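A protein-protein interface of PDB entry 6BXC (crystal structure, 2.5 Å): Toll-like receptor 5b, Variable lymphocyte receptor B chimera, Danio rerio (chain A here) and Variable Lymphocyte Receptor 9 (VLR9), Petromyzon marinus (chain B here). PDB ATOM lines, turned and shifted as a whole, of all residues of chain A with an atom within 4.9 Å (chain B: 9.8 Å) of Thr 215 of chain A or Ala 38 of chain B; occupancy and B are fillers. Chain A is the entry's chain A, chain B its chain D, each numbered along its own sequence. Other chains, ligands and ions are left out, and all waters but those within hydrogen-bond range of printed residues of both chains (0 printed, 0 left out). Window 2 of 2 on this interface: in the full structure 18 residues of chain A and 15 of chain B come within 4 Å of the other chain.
Among the printed residues, pairs that only touch across the chains: Gln 242 of chain A with Ala 38 of chain B, Thr 183 of chain A with Ser 39 of chain B, Gln 242 of chain A with Gln 57 of chain B and Thr 215 of chain A with Ala 38 of chain B.
The side-chain amide oxygen (OE1) of Gln 242 of chain A sits at hydrogen-bond distance from the side-chain hydroxyl (OG1) of Thr 59 of chain B, 2.5 Å away. The side-chain carboxylate of Glu 62 of chain B lies close to a ring nitrogen (NE2) of His 181 of chain A, 3.3 Å away.
Of chain B, only Ala 38 (3.96 Å) comes within 4 Å of Thr 215 of chain A. Ala 38 of chain B touches just these residues of chain A: Thr 215 and Gln 242. No residue of chain B comes within 4 Å of Thr 216 of chain A. Gln 242 of chain A touches three residues of chain B. No residue of chain B comes within 4 Å of Ser 243 of chain A. Of the printed residues of chain A, Ser 39 of chain B touches Thr 183 (3.7 Å). Of the printed residues of chain B, His 181 of chain A touches Glu 62 (2.9 Å). Of the printed residues of chain A, Thr 59 of chain B touches Gln 242 (2.5 Å). Printed residues of chain A within 4 Å of Glu 62 of chain B: His 181. Asn 80 of chain B touches none of the printed residues of chain A. Leu 37 of chain B touches none of the printed residues of chain A.
N of Gln 242 of chain A lies within hydrogen-bond range of O of Ile 214 of chain A (3.3 Å). The backbone carbonyl oxygen (O) of Thr 215 of chain A lies within hydrogen-bond range of the backbone NH (N) of Ser 243 of chain A (2.7 Å). N of Gln 242 of chain A sits at hydrogen-bond distance from O of Thr 215 of chain A, at 3.2 Å. The side-chain amide oxygen (OE1) of Gln 81 of chain B lies close to the backbone carbonyl oxygen (O) of Gln 57 of chain B, at 3.2 Å. The backbone carbonyl oxygen of Thr 183 of chain A sits at hydrogen-bond distance from the backbone NH of Thr 216 of chain A. N of Thr 215 of chain A is in hydrogen-bond range of O of Phe 182 of chain A, 2.9 Å away.
Of the 23 printed residues of chain B, 5 touch a printed residue of chain A. Printed residues of chain B that touch a printed residue of chain A: Ala 38, Ser 39, Gln 57, Thr 59 and Glu 62. Hydrophobic or aromatic side chains of chain B that line the printed part of chain A: Ala 38. Of the 11 printed residues of chain A, 4 touch a printed residue of chain B. Among the printed residues, no Asp or Glu carboxylate lies within 4 Å of a Lys or Arg side-chain nitrogen of the other chain.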
ATOM      1  N   HIS A 181       9.998  19.454  -7.087  1.00  0.00           N
ATOM      2  CA  HIS A 181       8.979  19.477  -6.043  1.00  0.00           C
ATOM      3  C   HIS A 181       9.674  19.270  -4.700  1.00  0.00           C
ATOM      4  O   HIS A 181      10.252  18.210  -4.455  1.00  0.00           O
ATOM      5  CB  HIS A 181       7.921  18.401  -6.231  1.00  0.00           C
ATOM      6  CG  HIS A 181       6.976  18.329  -5.077  1.00  0.00           C
ATOM      7  ND1 HIS A 181       6.023  19.296  -4.846  1.00  0.00           N
ATOM      8  CD2 HIS A 181       6.922  17.489  -4.017  1.00  0.00           C
ATOM      9  CE1 HIS A 181       5.365  19.010  -3.737  1.00  0.00           C
ATOM     10  NE2 HIS A 181       5.893  17.918  -3.213  1.00  0.00           N
ATOM     11  N   PHE A 182       9.674  20.298  -3.859  1.00  0.00           N
ATOM     12  CA  PHE A 182      10.220  20.186  -2.513  1.00  0.00           C
ATOM     13  C   PHE A 182       9.120  19.675  -1.588  1.00  0.00           C
ATOM     14  O   PHE A 182       7.984  20.154  -1.657  1.00  0.00           O
ATOM     15  CB  PHE A 182      10.734  21.543  -2.022  1.00  0.00           C
ATOM     16  CG  PHE A 182      11.990  22.013  -2.722  1.00  0.00           C
ATOM     17  CD1 PHE A 182      13.246  21.628  -2.279  1.00  0.00           C
ATOM     18  CD2 PHE A 182      11.903  22.872  -3.801  1.00  0.00           C
ATOM     19  CE1 PHE A 182      14.387  22.064  -2.919  1.00  0.00           C
ATOM     20  CE2 PHE A 182      13.044  23.320  -4.450  1.00  0.00           C
ATOM     21  CZ  PHE A 182      14.288  22.916  -4.009  1.00  0.00           C
ATOM     22  N   THR A 183       9.437  18.691  -0.740  1.00  0.00           N
ATOM     23  CA  THR A 183       8.463  18.321   0.284  1.00  0.00           C
ATOM     24  C   THR A 183       8.523  19.279   1.458  1.00  0.00           C
ATOM     25  O   THR A 183       7.498  19.574   2.070  1.00  0.00           O
ATOM     26  CB  THR A 183       8.688  16.896   0.803  1.00  0.00           C
ATOM     27  OG1 THR A 183      10.005  16.783   1.357  1.00  0.00           O
ATOM     28  CG2 THR A 183       8.517  15.870  -0.307  1.00  0.00           C
ATOM     29  N   SER A 213       6.967  23.413  -7.053  1.00  0.00           N
ATOM     30  CA  SER A 213       5.901  23.140  -6.110  1.00  0.00           C
ATOM     31  C   SER A 213       6.518  22.716  -4.787  1.00  0.00           C
ATOM     32  O   SER A 213       7.625  22.171  -4.744  1.00  0.00           O
ATOM     33  CB  SER A 213       4.959  22.065  -6.650  1.00  0.00           C
ATOM     34  OG  SER A 213       5.654  20.858  -6.900  1.00  0.00           O
ATOM     35  N   ILE A 214       5.796  22.992  -3.704  1.00  0.00           N
ATOM     36  CA  ILE A 214       6.294  22.812  -2.345  1.00  0.00           C
ATOM     37  C   ILE A 214       5.163  22.260  -1.500  1.00  0.00           C
ATOM     38  O   ILE A 214       4.069  22.830  -1.479  1.00  0.00           O
ATOM     39  CB  ILE A 214       6.814  24.126  -1.732  1.00  0.00           C
ATOM     40  CG1 ILE A 214       7.859  24.794  -2.633  1.00  0.00           C
ATOM     41  CG2 ILE A 214       7.387  23.868  -0.359  1.00  0.00           C
ATOM     42  CD1 ILE A 214       8.051  26.274  -2.337  1.00  0.00           C
ATOM     43  N   THR A 215       5.423  21.158  -0.798  1.00  0.00           N
ATOM     44  CA  THR A 215       4.430  20.614   0.125  1.00  0.00           C
ATOM     45  C   THR A 215       4.325  21.476   1.378  1.00  0.00           C
ATOM     46  O   THR A 215       3.253  22.010   1.693  1.00  0.00           O
ATOM     47  CB  THR A 215       4.776  19.167   0.476  1.00  0.00           C
ATOM     48  OG1 THR A 215       4.810  18.382  -0.722  1.00  0.00           O
ATOM     49  CG2 THR A 215       3.725  18.583   1.388  1.00  0.00           C
ATOM     50  N   THR A 216       5.428  21.612   2.115  1.00  0.00           N
ATOM     51  CA  THR A 216       5.480  22.460   3.299  1.00  0.00           C
ATOM     52  C   THR A 216       6.466  23.588   3.034  1.00  0.00           C
ATOM     53  O   THR A 216       7.657  23.337   2.822  1.00  0.00           O
ATOM     54  CB  THR A 216       5.908  21.654   4.525  1.00  0.00           C
ATOM     55  OG1 THR A 216       4.984  20.581   4.739  1.00  0.00           O
ATOM     56  CG2 THR A 216       5.964  22.549   5.763  1.00  0.00           C
ATOM     57  N   LEU A 217       5.956  24.820   2.986  1.00  0.00           N
ATOM     58  CA  LEU A 217       6.778  26.019   2.878  1.00  0.00           C
ATOM     59  C   LEU A 217       6.850  26.681   4.249  1.00  0.00           C
ATOM     60  O   LEU A 217       5.852  27.242   4.713  1.00  0.00           O
ATOM     61  CB  LEU A 217       6.193  26.961   1.832  1.00  0.00           C
ATOM     62  CG  LEU A 217       6.856  28.319   1.612  1.00  0.00           C
ATOM     63  CD1 LEU A 217       8.341  28.153   1.314  1.00  0.00           C
ATOM     64  CD2 LEU A 217       6.146  29.050   0.489  1.00  0.00           C
ATOM     65  N   ILE A 241       1.334  25.131  -3.034  1.00  0.00           N
ATOM     66  CA  ILE A 241       1.808  24.955  -1.665  1.00  0.00           C
ATOM     67  C   ILE A 241       0.692  24.307  -0.856  1.00  0.00           C
ATOM     68  O   ILE A 241      -0.424  24.835  -0.807  1.00  0.00           O
ATOM     69  CB  ILE A 241       2.229  26.292  -1.019  1.00  0.00           C
ATOM     70  CG1 ILE A 241       3.303  26.992  -1.848  1.00  0.00           C
ATOM     71  CG2 ILE A 241       2.762  26.060   0.392  1.00  0.00           C
ATOM     72  CD1 ILE A 241       3.366  28.487  -1.618  1.00  0.00           C
ATOM     73  N   GLN A 242       0.999  23.189  -0.192  1.00  0.00           N
ATOM     74  CA  GLN A 242      -0.022  22.496   0.584  1.00  0.00           C
ATOM     75  C   GLN A 242      -0.096  23.002   2.011  1.00  0.00           C
ATOM     76  O   GLN A 242      -1.200  23.174   2.544  1.00  0.00           O
ATOM     77  CB  GLN A 242       0.220  20.984   0.601  1.00  0.00           C
ATOM     78  CG  GLN A 242      -0.825  20.231   1.447  1.00  0.00           C
ATOM     79  CD  GLN A 242      -0.725  18.711   1.367  1.00  0.00           C
ATOM     80  OE1 GLN A 242      -1.149  18.109   0.388  1.00  0.00           O
ATOM     81  NE2 GLN A 242      -0.173  18.091   2.399  1.00  0.00           N
ATOM     82  N   SER A 243       1.050  23.243   2.645  1.00  0.00           N
ATOM     83  CA  SER A 243       1.087  23.782   4.000  1.00  0.00           C
ATOM     84  C   SER A 243       1.973  25.013   4.032  1.00  0.00           C
ATOM     85  O   SER A 243       3.161  24.933   3.711  1.00  0.00           O
ATOM     86  CB  SER A 243       1.603  22.737   4.994  1.00  0.00           C
ATOM     87  OG  SER A 243       2.122  23.365   6.150  1.00  0.00           O
ATOM     88  N   GLN B  22      10.366  12.491  13.374  1.00  0.00           N
ATOM     89  CA  GLN B  22       8.910  12.436  13.428  1.00  0.00           C
ATOM     90  C   GLN B  22       8.382  11.027  13.653  1.00  0.00           C
ATOM     91  O   GLN B  22       7.181  10.860  13.902  1.00  0.00           O
ATOM     92  CB  GLN B  22       8.348  12.984  12.116  1.00  0.00           C
ATOM     93  CG  GLN B  22       8.507  14.484  11.953  1.00  0.00           C
ATOM     94  CD  GLN B  22       8.515  14.910  10.495  1.00  0.00           C
ATOM     95  OE1 GLN B  22       9.085  14.222   9.645  1.00  0.00           O
ATOM     96  NE2 GLN B  22       7.896  16.049  10.200  1.00  0.00           N
ATOM     97  N   CYS B  32       5.715   5.752  11.535  1.00  0.00           N
ATOM     98  CA  CYS B  32       5.422   7.156  11.280  1.00  0.00           C
ATOM     99  C   CYS B  32       3.926   7.454  11.301  1.00  0.00           C
ATOM    100  O   CYS B  32       3.487   8.470  10.752  1.00  0.00           O
ATOM    101  CB  CYS B  32       6.030   7.583   9.937  1.00  0.00           C
ATOM    102  SG  CYS B  32       7.816   7.264   9.756  1.00  0.00           S
ATOM    103  N   GLY B  34       0.070   8.395  12.592  1.00  0.00           N
ATOM    104  CA  GLY B  34      -0.635   9.278  13.500  1.00  0.00           C
ATOM    105  C   GLY B  34       0.149  10.510  13.890  1.00  0.00           C
ATOM    106  O   GLY B  34      -0.024  11.025  15.000  1.00  0.00           O
ATOM    107  N   LYS B  35       0.983  11.025  12.984  1.00  0.00           N
ATOM    108  CA  LYS B  35       1.867  12.144  13.292  1.00  0.00           C
ATOM    109  C   LYS B  35       1.568  13.345  12.406  1.00  0.00           C
ATOM    110  O   LYS B  35       2.448  14.179  12.186  1.00  0.00           O
ATOM    111  CB  LYS B  35       3.333  11.731  13.132  1.00  0.00           C
ATOM    112  CG  LYS B  35       3.912  10.989  14.330  1.00  0.00           C
ATOM    113  CD  LYS B  35       3.918  11.818  15.608  1.00  0.00           C
ATOM    114  CE  LYS B  35       4.584  11.023  16.707  1.00  0.00           C
ATOM    115  NZ  LYS B  35       5.422   9.947  16.105  1.00  0.00           N
ATOM    116  N   SER B  36       0.342  13.431  11.887  1.00  0.00           N
ATOM    117  CA  SER B  36      -0.107  14.548  11.060  1.00  0.00           C
ATOM    118  C   SER B  36       0.857  14.826   9.908  1.00  0.00           C
ATOM    119  O   SER B  36       1.037  15.971   9.496  1.00  0.00           O
ATOM    120  CB  SER B  36      -0.315  15.798  11.920  1.00  0.00           C
ATOM    121  OG  SER B  36      -1.198  15.528  13.007  1.00  0.00           O
ATOM    122  N   LEU B  37       1.473  13.782   9.359  1.00  0.00           N
ATOM    123  CA  LEU B  37       2.468  13.974   8.310  1.00  0.00           C
ATOM    124  C   LEU B  37       1.828  14.282   6.959  1.00  0.00           C
ATOM    125  O   LEU B  37       0.873  13.618   6.542  1.00  0.00           O
ATOM    126  CB  LEU B  37       3.357  12.739   8.190  1.00  0.00           C
ATOM    127  CG  LEU B  37       4.168  12.410   9.438  1.00  0.00           C
ATOM    128  CD1 LEU B  37       4.999  11.167   9.173  1.00  0.00           C
ATOM    129  CD2 LEU B  37       5.050  13.607   9.774  1.00  0.00           C
ATOM    130  N   ALA B  38       2.406  15.269   6.252  1.00  0.00           N
ATOM    131  CA  ALA B  38       1.981  15.601   4.901  1.00  0.00           C
ATOM    132  C   ALA B  38       2.787  14.893   3.826  1.00  0.00           C
ATOM    133  O   ALA B  38       2.334  14.835   2.680  1.00  0.00           O
ATOM    134  CB  ALA B  38       2.072  17.109   4.671  1.00  0.00           C
ATOM    135  N   SER B  39       3.946  14.331   4.165  1.00  0.00           N
ATOM    136  CA  SER B  39       4.775  13.644   3.184  1.00  0.00           C
ATOM    137  C   SER B  39       5.529  12.526   3.891  1.00  0.00           C
ATOM    138  O   SER B  39       5.623  12.487   5.119  1.00  0.00           O
ATOM    139  CB  SER B  39       5.737  14.601   2.460  1.00  0.00           C
ATOM    140  OG  SER B  39       6.602  15.274   3.356  1.00  0.00           O
ATOM    141  N   VAL B  40       6.099  11.635   3.095  1.00  0.00           N
ATOM    142  CA  VAL B  40       6.891  10.526   3.641  1.00  0.00           C
ATOM    143  C   VAL B  40       8.197  11.064   4.214  1.00  0.00           C
ATOM    144  O   VAL B  40       8.887  11.848   3.546  1.00  0.00           O
ATOM    145  CB  VAL B  40       7.140   9.481   2.562  1.00  0.00           C
ATOM    146  CG1 VAL B  40       8.005   8.365   3.105  1.00  0.00           C
ATOM    147  CG2 VAL B  40       5.815   8.939   2.080  1.00  0.00           C
ATOM    148  N   PRO B  41       8.568  10.698   5.435  1.00  0.00           N
ATOM    149  CA  PRO B  41       9.839  11.179   5.988  1.00  0.00           C
ATOM    150  C   PRO B  41      11.036  10.669   5.199  1.00  0.00           C
ATOM    151  O   PRO B  41      11.034   9.558   4.664  1.00  0.00           O
ATOM    152  CB  PRO B  41       9.838  10.615   7.414  1.00  0.00           C
ATOM    153  CG  PRO B  41       8.389  10.426   7.740  1.00  0.00           C
ATOM    154  CD  PRO B  41       7.759   9.990   6.445  1.00  0.00           C
ATOM    155  N   LEU B  53       2.801   4.086   7.802  1.00  0.00           N
ATOM    156  CA  LEU B  53       2.534   5.469   7.429  1.00  0.00           C
ATOM    157  C   LEU B  53       1.058   5.847   7.536  1.00  0.00           C
ATOM    158  O   LEU B  53       0.660   6.879   6.987  1.00  0.00           O
ATOM    159  CB  LEU B  53       3.033   5.722   5.997  1.00  0.00           C
ATOM    160  CG  LEU B  53       4.541   5.857   5.752  1.00  0.00           C
ATOM    161  CD1 LEU B  53       4.881   5.582   4.312  1.00  0.00           C
ATOM    162  CD2 LEU B  53       4.988   7.265   6.107  1.00  0.00           C
ATOM    163  N   ASP B  55      -2.850   6.881   8.885  1.00  0.00           N
ATOM    164  CA  ASP B  55      -3.451   7.970   9.660  1.00  0.00           C
ATOM    165  C   ASP B  55      -2.553   9.212   9.652  1.00  0.00           C
ATOM    166  O   ASP B  55      -2.098   9.702  10.688  1.00  0.00           O
ATOM    167  CB  ASP B  55      -3.761   7.518  11.094  1.00  0.00           C
ATOM    168  CG  ASP B  55      -4.538   8.566  11.901  1.00  0.00           C
ATOM    169  OD1 ASP B  55      -5.259   9.392  11.303  1.00  0.00           O
ATOM    170  OD2 ASP B  55      -4.415   8.560  13.144  1.00  0.00           O
ATOM    171  N   ASN B  56      -2.309   9.721   8.448  1.00  0.00           N
ATOM    172  CA  ASN B  56      -1.589  10.977   8.257  1.00  0.00           C
ATOM    173  C   ASN B  56      -2.386  11.817   7.259  1.00  0.00           C
ATOM    174  O   ASN B  56      -3.579  11.594   7.019  1.00  0.00           O
ATOM    175  CB  ASN B  56      -0.135  10.713   7.839  1.00  0.00           C
ATOM    176  CG  ASN B  56       0.750  10.310   9.015  1.00  0.00           C
ATOM    177  OD1 ASN B  56       0.882  11.047   9.998  1.00  0.00           O
ATOM    178  ND2 ASN B  56       1.349   9.140   8.925  1.00  0.00           N
ATOM    179  N   GLN B  57      -1.739  12.809   6.656  1.00  0.00           N
ATOM    180  CA  GLN B  57      -2.401  13.652   5.663  1.00  0.00           C
ATOM    181  C   GLN B  57      -1.598  13.693   4.366  1.00  0.00           C
ATOM    182  O   GLN B  57      -1.496  14.730   3.704  1.00  0.00           O
ATOM    183  CB  GLN B  57      -2.615  15.059   6.218  1.00  0.00           C
ATOM    184  CG  GLN B  57      -3.636  15.117   7.356  1.00  0.00           C
ATOM    185  CD  GLN B  57      -3.712  16.475   8.041  1.00  0.00           C
ATOM    186  OE1 GLN B  57      -3.777  17.516   7.390  1.00  0.00           O
ATOM    187  NE2 GLN B  57      -3.710  16.465   9.370  1.00  0.00           N
ATOM    188  N   ILE B  58      -1.062  12.546   3.960  1.00  0.00           N
ATOM    189  CA  ILE B  58      -0.214  12.467   2.777  1.00  0.00           C
ATOM    190  C   ILE B  58      -1.102  12.531   1.541  1.00  0.00           C
ATOM    191  O   ILE B  58      -2.036  11.737   1.404  1.00  0.00           O
ATOM    192  CB  ILE B  58       0.614  11.178   2.798  1.00  0.00           C
ATOM    193  CG1 ILE B  58       1.527  11.174   4.029  1.00  0.00           C
ATOM    194  CG2 ILE B  58       1.446  11.064   1.511  1.00  0.00           C
ATOM    195  CD1 ILE B  58       2.203   9.848   4.305  1.00  0.00           C
ATOM    196  N   THR B  59      -0.838  13.494   0.656  1.00  0.00           N
ATOM    197  CA  THR B  59      -1.685  13.658  -0.520  1.00  0.00           C
ATOM    198  C   THR B  59      -1.064  13.120  -1.804  1.00  0.00           C
ATOM    199  O   THR B  59      -1.801  12.868  -2.763  1.00  0.00           O
ATOM    200  CB  THR B  59      -2.049  15.133  -0.721  1.00  0.00           C
ATOM    201  OG1 THR B  59      -0.853  15.920  -0.723  1.00  0.00           O
ATOM    202  CG2 THR B  59      -2.983  15.615   0.379  1.00  0.00           C
ATOM    203  N   LYS B  60       0.249  12.889  -1.838  1.00  0.00           N
ATOM    204  CA  LYS B  60       0.876  12.336  -3.033  1.00  0.00           C
ATOM    205  C   LYS B  60       2.155  11.643  -2.601  1.00  0.00           C
ATOM    206  O   LYS B  60       2.745  11.981  -1.571  1.00  0.00           O
ATOM    207  CB  LYS B  60       1.174  13.403  -4.096  1.00  0.00           C
ATOM    208  CG  LYS B  60       2.180  14.464  -3.684  1.00  0.00           C
ATOM    209  N   LEU B  61       2.624  10.732  -3.450  1.00  0.00           N
ATOM    210  CA  LEU B  61       3.942  10.133  -3.320  1.00  0.00           C
ATOM    211  C   LEU B  61       4.843  10.594  -4.456  1.00  0.00           C
ATOM    212  O   LEU B  61       4.417  10.645  -5.613  1.00  0.00           O
ATOM    213  CB  LEU B  61       3.833   8.604  -3.305  1.00  0.00           C
ATOM    214  CG  LEU B  61       2.922   7.985  -2.221  1.00  0.00           C
ATOM    215  CD1 LEU B  61       2.833   6.466  -2.366  1.00  0.00           C
ATOM    216  CD2 LEU B  61       3.339   8.353  -0.795  1.00  0.00           C
ATOM    217  N   GLU B  62       6.045  10.969  -4.122  1.00  0.00           N
ATOM    218  CA  GLU B  62       7.038  11.310  -5.118  1.00  0.00           C
ATOM    219  C   GLU B  62       7.574  10.045  -5.783  1.00  0.00           C
ATOM    220  O   GLU B  62       7.675   9.001  -5.131  1.00  0.00           O
ATOM    221  CB  GLU B  62       8.163  12.137  -4.506  1.00  0.00           C
ATOM    222  CG  GLU B  62       7.637  13.433  -3.922  1.00  0.00           C
ATOM    223  CD  GLU B  62       6.831  14.243  -4.942  1.00  0.00           C
ATOM    224  OE1 GLU B  62       7.157  14.208  -6.155  1.00  0.00           O
ATOM    225  OE2 GLU B  62       5.832  14.876  -4.536  1.00  0.00           O
ATOM    226  N   ILE B  79      -5.683   5.428   5.414  1.00  0.00           N
ATOM    227  CA  ILE B  79      -6.116   6.646   6.100  1.00  0.00           C
ATOM    228  C   ILE B  79      -5.163   7.774   5.733  1.00  0.00           C
ATOM    229  O   ILE B  79      -4.441   8.312   6.580  1.00  0.00           O
ATOM    230  CB  ILE B  79      -6.204   6.469   7.633  1.00  0.00           C
ATOM    231  CG1 ILE B  79      -6.926   5.169   7.989  1.00  0.00           C
ATOM    232  CG2 ILE B  79      -6.928   7.651   8.284  1.00  0.00           C
ATOM    233  CD1 ILE B  79      -6.855   4.804   9.460  1.00  0.00           C
ATOM    234  N   ASN B  80      -5.145   8.115   4.452  1.00  0.00           N
ATOM    235  CA  ASN B  80      -4.428   9.276   3.955  1.00  0.00           C
ATOM    236  C   ASN B  80      -5.334   9.922   2.919  1.00  0.00           C
ATOM    237  O   ASN B  80      -6.549   9.694   2.900  1.00  0.00           O
ATOM    238  CB  ASN B  80      -3.055   8.885   3.400  1.00  0.00           C
ATOM    239  CG  ASN B  80      -1.992   8.859   4.468  1.00  0.00           C
ATOM    240  OD1 ASN B  80      -1.649   9.893   5.051  1.00  0.00           O
ATOM    241  ND2 ASN B  80      -1.458   7.676   4.734  1.00  0.00           N
ATOM    242  N   GLN B  81      -4.763  10.776   2.083  1.00  0.00           N
ATOM    243  CA  GLN B  81      -5.517  11.510   1.076  1.00  0.00           C
ATOM    244  C   GLN B  81      -4.896  11.327  -0.299  1.00  0.00           C
ATOM    245  O   GLN B  81      -4.908  12.243  -1.126  1.00  0.00           O
ATOM    246  CB  GLN B  81      -5.659  12.986   1.446  1.00  0.00           C
ATOM    247  CG  GLN B  81      -6.425  13.206   2.744  1.00  0.00           C
ATOM    248  CD  GLN B  81      -5.596  13.826   3.843  1.00  0.00           C
ATOM    249  OE1 GLN B  81      -4.654  14.572   3.580  1.00  0.00           O
ATOM    250  NE2 GLN B  81      -5.944  13.521   5.089  1.00  0.00           N
ATOM    251  N   LEU B  82      -4.373  10.133  -0.582  1.00  0.00           N
ATOM    252  CA  LEU B  82      -3.698   9.906  -1.853  1.00  0.00           C
ATOM    253  C   LEU B  82      -4.716   9.967  -2.984  1.00  0.00           C
ATOM    254  O   LEU B  82      -5.738   9.278  -2.943  1.00  0.00           O
ATOM    255  CB  LEU B  82      -3.020   8.536  -1.842  1.00  0.00           C
ATOM    256  CG  LEU B  82      -1.876   8.338  -0.845  1.00  0.00           C
ATOM    257  CD1 LEU B  82      -1.409   6.888  -0.831  1.00  0.00           C
ATOM    258  CD2 LEU B  82      -0.718   9.291  -1.088  1.00  0.00           C
